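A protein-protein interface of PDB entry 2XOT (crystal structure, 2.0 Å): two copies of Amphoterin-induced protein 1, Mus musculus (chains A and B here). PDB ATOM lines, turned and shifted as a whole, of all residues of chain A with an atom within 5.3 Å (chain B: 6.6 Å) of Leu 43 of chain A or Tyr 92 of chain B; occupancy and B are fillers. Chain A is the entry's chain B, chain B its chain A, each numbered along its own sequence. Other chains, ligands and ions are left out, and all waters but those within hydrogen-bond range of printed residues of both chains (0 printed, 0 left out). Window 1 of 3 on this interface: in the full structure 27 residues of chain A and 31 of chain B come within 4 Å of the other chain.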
ATOM      1  N   ASN A  21     -13.432   9.754 -23.742  1.00  0.00           N
ATOM      2  CA  ASN A  21     -14.588   9.183 -23.029  1.00  0.00           C
ATOM      3  C   ASN A  21     -14.257   8.453 -21.721  1.00  0.00           C
ATOM      4  O   ASN A  21     -15.131   7.846 -21.120  1.00  0.00           O
ATOM      5  CB  ASN A  21     -15.477   8.345 -23.969  1.00  0.00           C
ATOM      6  CG  ASN A  21     -14.816   7.077 -24.475  1.00  0.00           C
ATOM      7  OD1 ASN A  21     -13.693   6.744 -24.103  1.00  0.00           O
ATOM      8  ND2 ASN A  21     -15.546   6.326 -25.321  1.00  0.00           N
ATOM      9  N   ILE A  22     -13.023   8.571 -21.244  1.00  0.00           N
ATOM     10  CA  ILE A  22     -12.656   8.037 -19.930  1.00  0.00           C
ATOM     11  C   ILE A  22     -12.394   9.136 -18.874  1.00  0.00           C
ATOM     12  O   ILE A  22     -11.556  10.005 -19.084  1.00  0.00           O
ATOM     13  CB  ILE A  22     -11.389   7.180 -20.041  1.00  0.00           C
ATOM     14  CG1 ILE A  22     -11.696   5.914 -20.864  1.00  0.00           C
ATOM     15  CG2 ILE A  22     -10.835   6.820 -18.638  1.00  0.00           C
ATOM     16  CD1 ILE A  22     -10.520   4.986 -20.989  1.00  0.00           C
ATOM     17  N   LEU A  23     -13.108   9.088 -17.743  1.00  0.00           N
ATOM     18  CA  LEU A  23     -12.810   9.994 -16.620  1.00  0.00           C
ATOM     19  C   LEU A  23     -12.101   9.175 -15.580  1.00  0.00           C
ATOM     20  O   LEU A  23     -12.644   8.199 -15.112  1.00  0.00           O
ATOM     21  CB  LEU A  23     -14.072  10.586 -15.989  1.00  0.00           C
ATOM     22  CG  LEU A  23     -14.998  11.540 -16.756  1.00  0.00           C
ATOM     23  CD1 LEU A  23     -15.521  12.621 -15.812  1.00  0.00           C
ATOM     24  CD2 LEU A  23     -14.398  12.123 -18.034  1.00  0.00           C
ATOM     25  N   THR A  41     -19.243  10.314 -21.191  1.00  0.00           N
ATOM     26  CA  THR A  41     -18.447   9.384 -20.364  1.00  0.00           C
ATOM     27  C   THR A  41     -18.811   7.909 -20.596  1.00  0.00           C
ATOM     28  O   THR A  41     -20.006   7.509 -20.500  1.00  0.00           O
ATOM     29  CB  THR A  41     -18.560   9.730 -18.864  1.00  0.00           C
ATOM     30  OG1 THR A  41     -18.391  11.141 -18.692  1.00  0.00           O
ATOM     31  CG2 THR A  41     -17.490   9.040 -18.039  1.00  0.00           C
ATOM     32  N   ALA A  42     -17.778   7.120 -20.925  1.00  0.00           N
ATOM     33  CA  ALA A  42     -17.892   5.671 -21.149  1.00  0.00           C
ATOM     34  C   ALA A  42     -17.440   4.870 -19.916  1.00  0.00           C
ATOM     35  O   ALA A  42     -18.061   3.868 -19.570  1.00  0.00           O
ATOM     36  CB  ALA A  42     -17.046   5.245 -22.380  1.00  0.00           C
ATOM     37  N   LEU A  43     -16.331   5.291 -19.289  1.00  0.00           N
ATOM     38  CA  LEU A  43     -15.815   4.668 -18.054  1.00  0.00           C
ATOM     39  C   LEU A  43     -15.591   5.769 -17.045  1.00  0.00           C
ATOM     40  O   LEU A  43     -15.030   6.818 -17.377  1.00  0.00           O
ATOM     41  CB  LEU A  43     -14.513   3.902 -18.305  1.00  0.00           C
ATOM     42  CG  LEU A  43     -13.830   3.125 -17.168  1.00  0.00           C
ATOM     43  CD1 LEU A  43     -13.287   1.788 -17.677  1.00  0.00           C
ATOM     44  CD2 LEU A  43     -12.691   3.886 -16.558  1.00  0.00           C
ATOM     45  N   LEU A  44     -16.089   5.554 -15.836  1.00  0.00           N
ATOM     46  CA  LEU A  44     -15.906   6.482 -14.738  1.00  0.00           C
ATOM     47  C   LEU A  44     -15.235   5.759 -13.583  1.00  0.00           C
ATOM     48  O   LEU A  44     -15.806   4.804 -12.999  1.00  0.00           O
ATOM     49  CB  LEU A  44     -17.277   7.049 -14.353  1.00  0.00           C
ATOM     50  CG  LEU A  44     -17.345   8.002 -13.162  1.00  0.00           C
ATOM     51  CD1 LEU A  44     -16.353   9.144 -13.351  1.00  0.00           C
ATOM     52  CD2 LEU A  44     -18.793   8.480 -13.013  1.00  0.00           C
ATOM     53  N   ASP A  45     -14.019   6.193 -13.253  1.00  0.00           N
ATOM     54  CA  ASP A  45     -13.239   5.584 -12.166  1.00  0.00           C
ATOM     55  C   ASP A  45     -13.176   6.504 -10.966  1.00  0.00           C
ATOM     56  O   ASP A  45     -12.440   7.480 -11.015  1.00  0.00           O
ATOM     57  CB  ASP A  45     -11.801   5.298 -12.632  1.00  0.00           C
ATOM     58  CG  ASP A  45     -10.969   4.610 -11.576  1.00  0.00           C
ATOM     59  OD1 ASP A  45     -11.472   4.248 -10.489  1.00  0.00           O
ATOM     60  OD2 ASP A  45      -9.774   4.411 -11.845  1.00  0.00           O
ATOM     61  N   LEU A  66     -22.419   5.443 -20.340  1.00  0.00           N
ATOM     62  CA  LEU A  66     -21.549   4.827 -19.294  1.00  0.00           C
ATOM     63  C   LEU A  66     -21.675   3.308 -19.341  1.00  0.00           C
ATOM     64  O   LEU A  66     -22.766   2.786 -19.153  1.00  0.00           O
ATOM     65  CB  LEU A  66     -21.881   5.320 -17.862  1.00  0.00           C
ATOM     66  CG  LEU A  66     -20.783   5.122 -16.792  1.00  0.00           C
ATOM     67  CD1 LEU A  66     -19.559   5.957 -17.148  1.00  0.00           C
ATOM     68  CD2 LEU A  66     -21.186   5.462 -15.353  1.00  0.00           C
ATOM     69  N   HIS A  67     -20.564   2.608 -19.585  1.00  0.00           N
ATOM     70  CA  HIS A  67     -20.532   1.132 -19.534  1.00  0.00           C
ATOM     71  C   HIS A  67     -19.828   0.537 -18.315  1.00  0.00           C
ATOM     72  O   HIS A  67     -20.144  -0.575 -17.874  1.00  0.00           O
ATOM     73  CB  HIS A  67     -19.906   0.610 -20.809  1.00  0.00           C
ATOM     74  CG  HIS A  67     -20.733   0.895 -22.017  1.00  0.00           C
ATOM     75  ND1 HIS A  67     -20.247   0.772 -23.300  1.00  0.00           N
ATOM     76  CD2 HIS A  67     -22.022   1.309 -22.134  1.00  0.00           C
ATOM     77  CE1 HIS A  67     -21.201   1.098 -24.159  1.00  0.00           C
ATOM     78  NE2 HIS A  67     -22.289   1.428 -23.478  1.00  0.00           N
ATOM     79  N   SER A  68     -18.875   1.289 -17.765  1.00  0.00           N
ATOM     80  CA  SER A  68     -18.165   0.892 -16.553  1.00  0.00           C
ATOM     81  C   SER A  68     -18.181   1.956 -15.467  1.00  0.00           C
ATOM     82  O   SER A  68     -17.864   3.109 -15.722  1.00  0.00           O
ATOM     83  CB  SER A  68     -16.724   0.589 -16.918  1.00  0.00           C
ATOM     84  OG  SER A  68     -16.719  -0.498 -17.855  1.00  0.00           O
ATOM     85  N   LEU A  70     -16.634   2.332 -11.684  1.00  0.00           N
ATOM     86  CA  LEU A  70     -15.685   1.758 -10.766  1.00  0.00           C
ATOM     87  C   LEU A  70     -15.760   2.556  -9.475  1.00  0.00           C
ATOM     88  O   LEU A  70     -15.341   3.714  -9.461  1.00  0.00           O
ATOM     89  CB  LEU A  70     -14.268   1.855 -11.347  1.00  0.00           C
ATOM     90  CG  LEU A  70     -13.830   0.824 -12.395  1.00  0.00           C
ATOM     91  CD1 LEU A  70     -14.948   0.286 -13.230  1.00  0.00           C
ATOM     92  CD2 LEU A  70     -12.682   1.392 -13.278  1.00  0.00           C
ATOM     93  N   HIS B  67      -7.072 -11.738 -18.749  1.00  0.00           N
ATOM     94  CA  HIS B  67      -7.728 -10.891 -19.758  1.00  0.00           C
ATOM     95  C   HIS B  67      -7.548  -9.399 -19.504  1.00  0.00           C
ATOM     96  O   HIS B  67      -7.503  -8.620 -20.444  1.00  0.00           O
ATOM     97  CB  HIS B  67      -9.227 -11.261 -19.892  1.00  0.00           C
ATOM     98  CG  HIS B  67      -9.456 -12.605 -20.531  1.00  0.00           C
ATOM     99  ND1 HIS B  67     -10.672 -13.262 -20.495  1.00  0.00           N
ATOM    100  CD2 HIS B  67      -8.616 -13.412 -21.228  1.00  0.00           C
ATOM    101  CE1 HIS B  67     -10.572 -14.414 -21.147  1.00  0.00           C
ATOM    102  NE2 HIS B  67      -9.332 -14.528 -21.604  1.00  0.00           N
ATOM    103  N   SER B  68      -7.428  -9.008 -18.235  1.00  0.00           N
ATOM    104  CA  SER B  68      -7.209  -7.612 -17.868  1.00  0.00           C
ATOM    105  C   SER B  68      -5.999  -7.488 -16.976  1.00  0.00           C
ATOM    106  O   SER B  68      -5.874  -8.237 -16.028  1.00  0.00           O
ATOM    107  CB  SER B  68      -8.423  -7.064 -17.136  1.00  0.00           C
ATOM    108  OG  SER B  68      -9.579  -7.312 -17.913  1.00  0.00           O
ATOM    109  N   LEU B  69      -5.109  -6.568 -17.331  1.00  0.00           N
ATOM    110  CA  LEU B  69      -3.959  -6.187 -16.504  1.00  0.00           C
ATOM    111  C   LEU B  69      -4.017  -4.702 -16.261  1.00  0.00           C
ATOM    112  O   LEU B  69      -3.867  -3.910 -17.189  1.00  0.00           O
ATOM    113  CB  LEU B  69      -2.670  -6.521 -17.212  1.00  0.00           C
ATOM    114  CG  LEU B  69      -1.340  -6.141 -16.573  1.00  0.00           C
ATOM    115  CD1 LEU B  69      -1.209  -6.734 -15.146  1.00  0.00           C
ATOM    116  CD2 LEU B  69      -0.198  -6.600 -17.481  1.00  0.00           C
ATOM    117  N   LEU B  70      -4.207  -4.319 -15.003  1.00  0.00           N
ATOM    118  CA  LEU B  70      -4.354  -2.894 -14.630  1.00  0.00           C
ATOM    119  C   LEU B  70      -3.107  -2.440 -13.879  1.00  0.00           C
ATOM    120  O   LEU B  70      -2.823  -2.932 -12.781  1.00  0.00           O
ATOM    121  CB  LEU B  70      -5.608  -2.680 -13.778  1.00  0.00           C
ATOM    122  CG  LEU B  70      -6.885  -3.360 -14.345  1.00  0.00           C
ATOM    123  CD1 LEU B  70      -8.085  -3.202 -13.384  1.00  0.00           C
ATOM    124  CD2 LEU B  70      -7.223  -2.861 -15.760  1.00  0.00           C
ATOM    125  N   ASN B  89      -3.191 -13.974 -24.129  1.00  0.00           N
ATOM    126  CA  ASN B  89      -4.616 -13.797 -24.276  1.00  0.00           C
ATOM    127  C   ASN B  89      -5.158 -12.515 -23.672  1.00  0.00           C
ATOM    128  O   ASN B  89      -6.354 -12.340 -23.584  1.00  0.00           O
ATOM    129  CB  ASN B  89      -5.304 -15.041 -23.736  1.00  0.00           C
ATOM    130  CG  ASN B  89      -4.841 -16.281 -24.468  1.00  0.00           C
ATOM    131  OD1 ASN B  89      -4.521 -17.328 -23.880  1.00  0.00           O
ATOM    132  ND2 ASN B  89      -4.706 -16.133 -25.745  1.00  0.00           N
ATOM    133  N   LEU B  90      -4.268 -11.599 -23.328  1.00  0.00           N
ATOM    134  CA  LEU B  90      -4.670 -10.304 -22.748  1.00  0.00           C
ATOM    135  C   LEU B  90      -5.574  -9.495 -23.709  1.00  0.00           C
ATOM    136  O   LEU B  90      -5.315  -9.404 -24.900  1.00  0.00           O
ATOM    137  CB  LEU B  90      -3.429  -9.506 -22.323  1.00  0.00           C
ATOM    138  CG  LEU B  90      -3.610  -8.399 -21.290  1.00  0.00           C
ATOM    139  CD1 LEU B  90      -4.038  -8.978 -19.929  1.00  0.00           C
ATOM    140  CD2 LEU B  90      -2.314  -7.559 -21.202  1.00  0.00           C
ATOM    141  N   ARG B  91      -6.658  -8.950 -23.159  1.00  0.00           N
ATOM    142  CA  ARG B  91      -7.626  -8.171 -23.909  1.00  0.00           C
ATOM    143  C   ARG B  91      -7.638  -6.703 -23.549  1.00  0.00           C
ATOM    144  O   ARG B  91      -8.065  -5.908 -24.359  1.00  0.00           O
ATOM    145  CB  ARG B  91      -9.030  -8.684 -23.614  1.00  0.00           C
ATOM    146  CG  ARG B  91      -9.228 -10.095 -24.009  1.00  0.00           C
ATOM    147  CD  ARG B  91     -10.614 -10.560 -23.718  1.00  0.00           C
ATOM    148  NE  ARG B  91     -10.724 -11.955 -24.151  1.00  0.00           N
ATOM    149  CZ  ARG B  91     -11.754 -12.732 -23.881  1.00  0.00           C
ATOM    150  NH1 ARG B  91     -12.795 -12.259 -23.183  1.00  0.00           N
ATOM    151  NH2 ARG B  91     -11.735 -13.986 -24.311  1.00  0.00           N
ATOM    152  N   TYR B  92      -7.255  -6.377 -22.308  1.00  0.00           N
ATOM    153  CA  TYR B  92      -7.393  -5.029 -21.763  1.00  0.00           C
ATOM    154  C   TYR B  92      -6.149  -4.714 -20.935  1.00  0.00           C
ATOM    155  O   TYR B  92      -5.836  -5.449 -20.008  1.00  0.00           O
ATOM    156  CB  TYR B  92      -8.618  -4.970 -20.845  1.00  0.00           C
ATOM    157  CG  TYR B  92      -9.080  -3.566 -20.493  1.00  0.00           C
ATOM    158  CD1 TYR B  92     -10.089  -2.953 -21.214  1.00  0.00           C
ATOM    159  CD2 TYR B  92      -8.508  -2.864 -19.444  1.00  0.00           C
ATOM    160  CE1 TYR B  92     -10.542  -1.669 -20.889  1.00  0.00           C
ATOM    161  CE2 TYR B  92      -8.956  -1.554 -19.110  1.00  0.00           C
ATOM    162  CZ  TYR B  92      -9.961  -0.975 -19.848  1.00  0.00           C
ATOM    163  OH  TYR B  92     -10.414   0.295 -19.529  1.00  0.00           O
ATOM    164  N   LEU B  93      -5.470  -3.622 -21.264  1.00  0.00           N
ATOM    165  CA  LEU B  93      -4.212  -3.242 -20.628  1.00  0.00           C
ATOM    166  C   LEU B  93      -4.289  -1.747 -20.321  1.00  0.00           C
ATOM    167  O   LEU B  93      -4.444  -0.913 -21.231  1.00  0.00           O
ATOM    168  CB  LEU B  93      -3.036  -3.547 -21.549  1.00  0.00           C
ATOM    169  CG  LEU B  93      -1.601  -3.136 -21.175  1.00  0.00           C
ATOM    170  CD1 LEU B  93      -1.207  -3.706 -19.813  1.00  0.00           C
ATOM    171  CD2 LEU B  93      -0.637  -3.613 -22.248  1.00  0.00           C
ATOM    172  N   ASP B  94      -4.204  -1.429 -19.032  1.00  0.00           N
ATOM    173  CA  ASP B  94      -4.156  -0.053 -18.562  1.00  0.00           C
ATOM    174  C   ASP B  94      -2.752   0.310 -18.055  1.00  0.00           C
ATOM    175  O   ASP B  94      -2.314  -0.126 -16.967  1.00  0.00           O
ATOM    176  CB  ASP B  94      -5.195   0.158 -17.468  1.00  0.00           C
ATOM    177  CG  ASP B  94      -5.375   1.624 -17.118  1.00  0.00           C
ATOM    178  OD1 ASP B  94      -4.599   2.468 -17.638  1.00  0.00           O
ATOM    179  OD2 ASP B  94      -6.296   1.919 -16.334  1.00  0.00           O
ATOM    180  N   ALA B 113      -4.390 -10.328 -29.115  1.00  0.00           N
ATOM    181  CA  ALA B 113      -5.801 -10.408 -28.723  1.00  0.00           C
ATOM    182  C   ALA B 113      -6.290  -9.125 -28.016  1.00  0.00           C
ATOM    183  O   ALA B 113      -7.454  -9.034 -27.636  1.00  0.00           O
ATOM    184  CB  ALA B 113      -6.032 -11.628 -27.838  1.00  0.00           C
ATOM    185  N   LEU B 114      -5.407  -8.143 -27.856  1.00  0.00           N
ATOM    186  CA  LEU B 114      -5.712  -6.950 -27.066  1.00  0.00           C
ATOM    187  C   LEU B 114      -6.704  -6.120 -27.850  1.00  0.00           C
ATOM    188  O   LEU B 114      -6.524  -5.899 -29.045  1.00  0.00           O
ATOM    189  CB  LEU B 114      -4.448  -6.115 -26.783  1.00  0.00           C
ATOM    190  CG  LEU B 114      -4.546  -5.070 -25.674  1.00  0.00           C
ATOM    191  CD1 LEU B 114      -4.555  -5.750 -24.287  1.00  0.00           C
ATOM    192  CD2 LEU B 114      -3.395  -4.088 -25.761  1.00  0.00           C
ATOM    193  N   GLU B 115      -7.741  -5.676 -27.146  1.00  0.00           N
ATOM    194  CA  GLU B 115      -8.789  -4.837 -27.705  1.00  0.00           C
ATOM    195  C   GLU B 115      -8.729  -3.393 -27.246  1.00  0.00           C
ATOM    196  O   GLU B 115      -9.139  -2.491 -28.000  1.00  0.00           O
ATOM    197  CB  GLU B 115     -10.150  -5.409 -27.321  1.00  0.00           C
ATOM    198  CG  GLU B 115     -10.355  -6.822 -27.798  1.00  0.00           C
ATOM    199  CD  GLU B 115     -11.784  -7.279 -27.634  1.00  0.00           C
ATOM    200  OE1 GLU B 115     -12.327  -7.181 -26.502  1.00  0.00           O
ATOM    201  OE2 GLU B 115     -12.358  -7.734 -28.654  1.00  0.00           O
ATOM    202  N   VAL B 116      -8.210  -3.170 -26.037  1.00  0.00           N
ATOM    203  CA  VAL B 116      -8.114  -1.812 -25.470  1.00  0.00           C
ATOM    204  C   VAL B 116      -6.738  -1.596 -24.862  1.00  0.00           C
ATOM    205  O   VAL B 116      -6.302  -2.407 -24.044  1.00  0.00           O
ATOM    206  CB  VAL B 116      -9.193  -1.602 -24.375  1.00  0.00           C
ATOM    207  CG1 VAL B 116      -9.138  -0.151 -23.802  1.00  0.00           C
ATOM    208  CG2 VAL B 116     -10.628  -1.976 -24.898  1.00  0.00           C
ATOM    209  N   LEU B 117      -6.067  -0.518 -25.255  1.00  0.00           N
ATOM    210  CA  LEU B 117      -4.754  -0.130 -24.680  1.00  0.00           C
ATOM    211  C   LEU B 117      -4.837   1.315 -24.219  1.00  0.00           C
ATOM    212  O   LEU B 117      -5.086   2.227 -25.029  1.00  0.00           O
ATOM    213  CB  LEU B 117      -3.622  -0.258 -25.701  1.00  0.00           C
ATOM    214  CG  LEU B 117      -2.169   0.055 -25.289  1.00  0.00           C
ATOM    215  CD1 LEU B 117      -1.743  -0.596 -23.972  1.00  0.00           C
ATOM    216  CD2 LEU B 117      -1.195  -0.384 -26.387  1.00  0.00           C
ATOM    217  N   LEU B 118      -4.639   1.500 -22.914  1.00  0.00           N
ATOM    218  CA  LEU B 118      -4.656   2.823 -22.294  1.00  0.00           C
ATOM    219  C   LEU B 118      -3.242   3.214 -21.957  1.00  0.00           C
ATOM    220  O   LEU B 118      -2.585   2.533 -21.181  1.00  0.00           O
ATOM    221  CB  LEU B 118      -5.452   2.824 -20.988  1.00  0.00           C
ATOM    222  CG  LEU B 118      -6.973   2.755 -20.976  1.00  0.00           C
ATOM    223  CD1 LEU B 118      -7.514   1.916 -22.033  1.00  0.00           C
ATOM    224  CD2 LEU B 118      -7.490   2.281 -19.612  1.00  0.00           C
ATOM    225  N   TYR B 120      -2.651   6.870 -21.584  1.00  0.00           N
ATOM    226  CA  TYR B 120      -2.854   8.303 -21.454  1.00  0.00           C
ATOM    227  C   TYR B 120      -2.174   8.772 -20.186  1.00  0.00           C
ATOM    228  O   TYR B 120      -1.930   7.984 -19.270  1.00  0.00           O
ATOM    229  CB  TYR B 120      -4.325   8.670 -21.468  1.00  0.00           C
ATOM    230  CG  TYR B 120      -5.148   8.163 -20.296  1.00  0.00           C
ATOM    231  CD1 TYR B 120      -5.216   8.890 -19.102  1.00  0.00           C
ATOM    232  CD2 TYR B 120      -5.879   6.979 -20.381  1.00  0.00           C
ATOM    233  CE1 TYR B 120      -5.969   8.450 -18.034  1.00  0.00           C
ATOM    234  CE2 TYR B 120      -6.650   6.524 -19.292  1.00  0.00           C
ATOM    235  CZ  TYR B 120      -6.676   7.269 -18.122  1.00  0.00           C
ATOM    236  OH  TYR B 120      -7.405   6.847 -17.023  1.00  0.00           O
ATOM    237  N   TYR B 142      -5.783   4.735 -26.431  1.00  0.00           N
ATOM    238  CA  TYR B 142      -5.841   6.039 -25.740  1.00  0.00           C
ATOM    239  C   TYR B 142      -4.444   6.564 -25.483  1.00  0.00           C
ATOM    240  O   TYR B 142      -3.644   5.921 -24.771  1.00  0.00           O
ATOM    241  CB  TYR B 142      -6.564   5.898 -24.414  1.00  0.00           C
ATOM    242  CG  TYR B 142      -8.030   5.591 -24.521  1.00  0.00           C
ATOM    243  CD1 TYR B 142      -8.979   6.606 -24.440  1.00  0.00           C
ATOM    244  CD2 TYR B 142      -8.479   4.279 -24.630  1.00  0.00           C
ATOM    245  CE1 TYR B 142     -10.331   6.324 -24.477  1.00  0.00           C
ATOM    246  CE2 TYR B 142      -9.823   3.995 -24.704  1.00  0.00           C
ATOM    247  CZ  TYR B 142     -10.739   5.025 -24.629  1.00  0.00           C
ATOM    248  OH  TYR B 142     -12.077   4.748 -24.676  1.00  0.00           O
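Positions printed for both chains: 67, 68 and 70.
Among the printed residues, merely in contact across the chains: Ile 22 of chain A with Tyr 120 of chain B (3.8 Å), Ile 22 of chain A with Tyr 142 of chain B (3.6 Å) and Leu 43 of chain A with Tyr 92 of chain B (3.7 Å).
Leu 43 of chain A touches just one residue of chain B: Tyr 92 (3.7 Å).
Tyr 92 of chain B touches just one residue of chain A: Leu 43.
Printed residues of chain A within 4 Å of Tyr 142 of chain B: Asn 21 and Ile 22.
Printed residues of chain B within 4 Å of Asn 21 of chain A: Tyr 142 (2.6 Å).
Of the printed residues of chain A, Tyr 120 of chain B touches Ile 22.
Asp 45 of chain A touches none of the printed residues of chain B.
Asp 94 of chain B touches none of the printed residues of chain A.
The nearest residue of chain A that does not touch Tyr 92 of chain B is Ile 22 of chain A (4.9 Å).
The nearest printed residue of chain A that does not touch Tyr 142 of chain B is Ala 42 of chain A (5.5 Å).
The side-chain hydroxyl (OH) of Tyr 142 of chain B sits at hydrogen-bond distance from the side-chain amide oxygen (OD1) of Asn 21 of chain A (2.6 Å).
Of the 18 printed residues of chain B, 3 touch a printed residue of chain A.
Hydrophobic or aromatic side chains of chain B within 4 Å of the printed part of chain A: Tyr 92, Tyr 120 and Tyr 142.
Along chain A the printed residues that touch a printed residue of chain B span positions 21 to 43.
Among the printed residues, 4 pairs touch across the chains.
The backbone carbonyl oxygen (O) of Asn 21 of chain A is in hydrogen-bond range of the backbone NH (N) of Leu 43 of chain A.
N of Tyr 120 of chain B is in hydrogen-bond range of O of Tyr 142 of chain B (3.5 Å).
N of Leu 23 of chain A sits at hydrogen-bond distance from O of Leu 43 of chain A (3.0 Å).
O of Asn 21 of chain A lies within hydrogen-bond range of N of Ala 42 of chain A (2.8 Å).
The backbone NH (N) of Leu 69 of chain B lies within hydrogen-bond range of the backbone carbonyl oxygen (O) of Tyr 92 of chain B.
O of Leu 117 of chain B sits at hydrogen-bond distance from N of Tyr 142 of chain B (3.0 Å).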
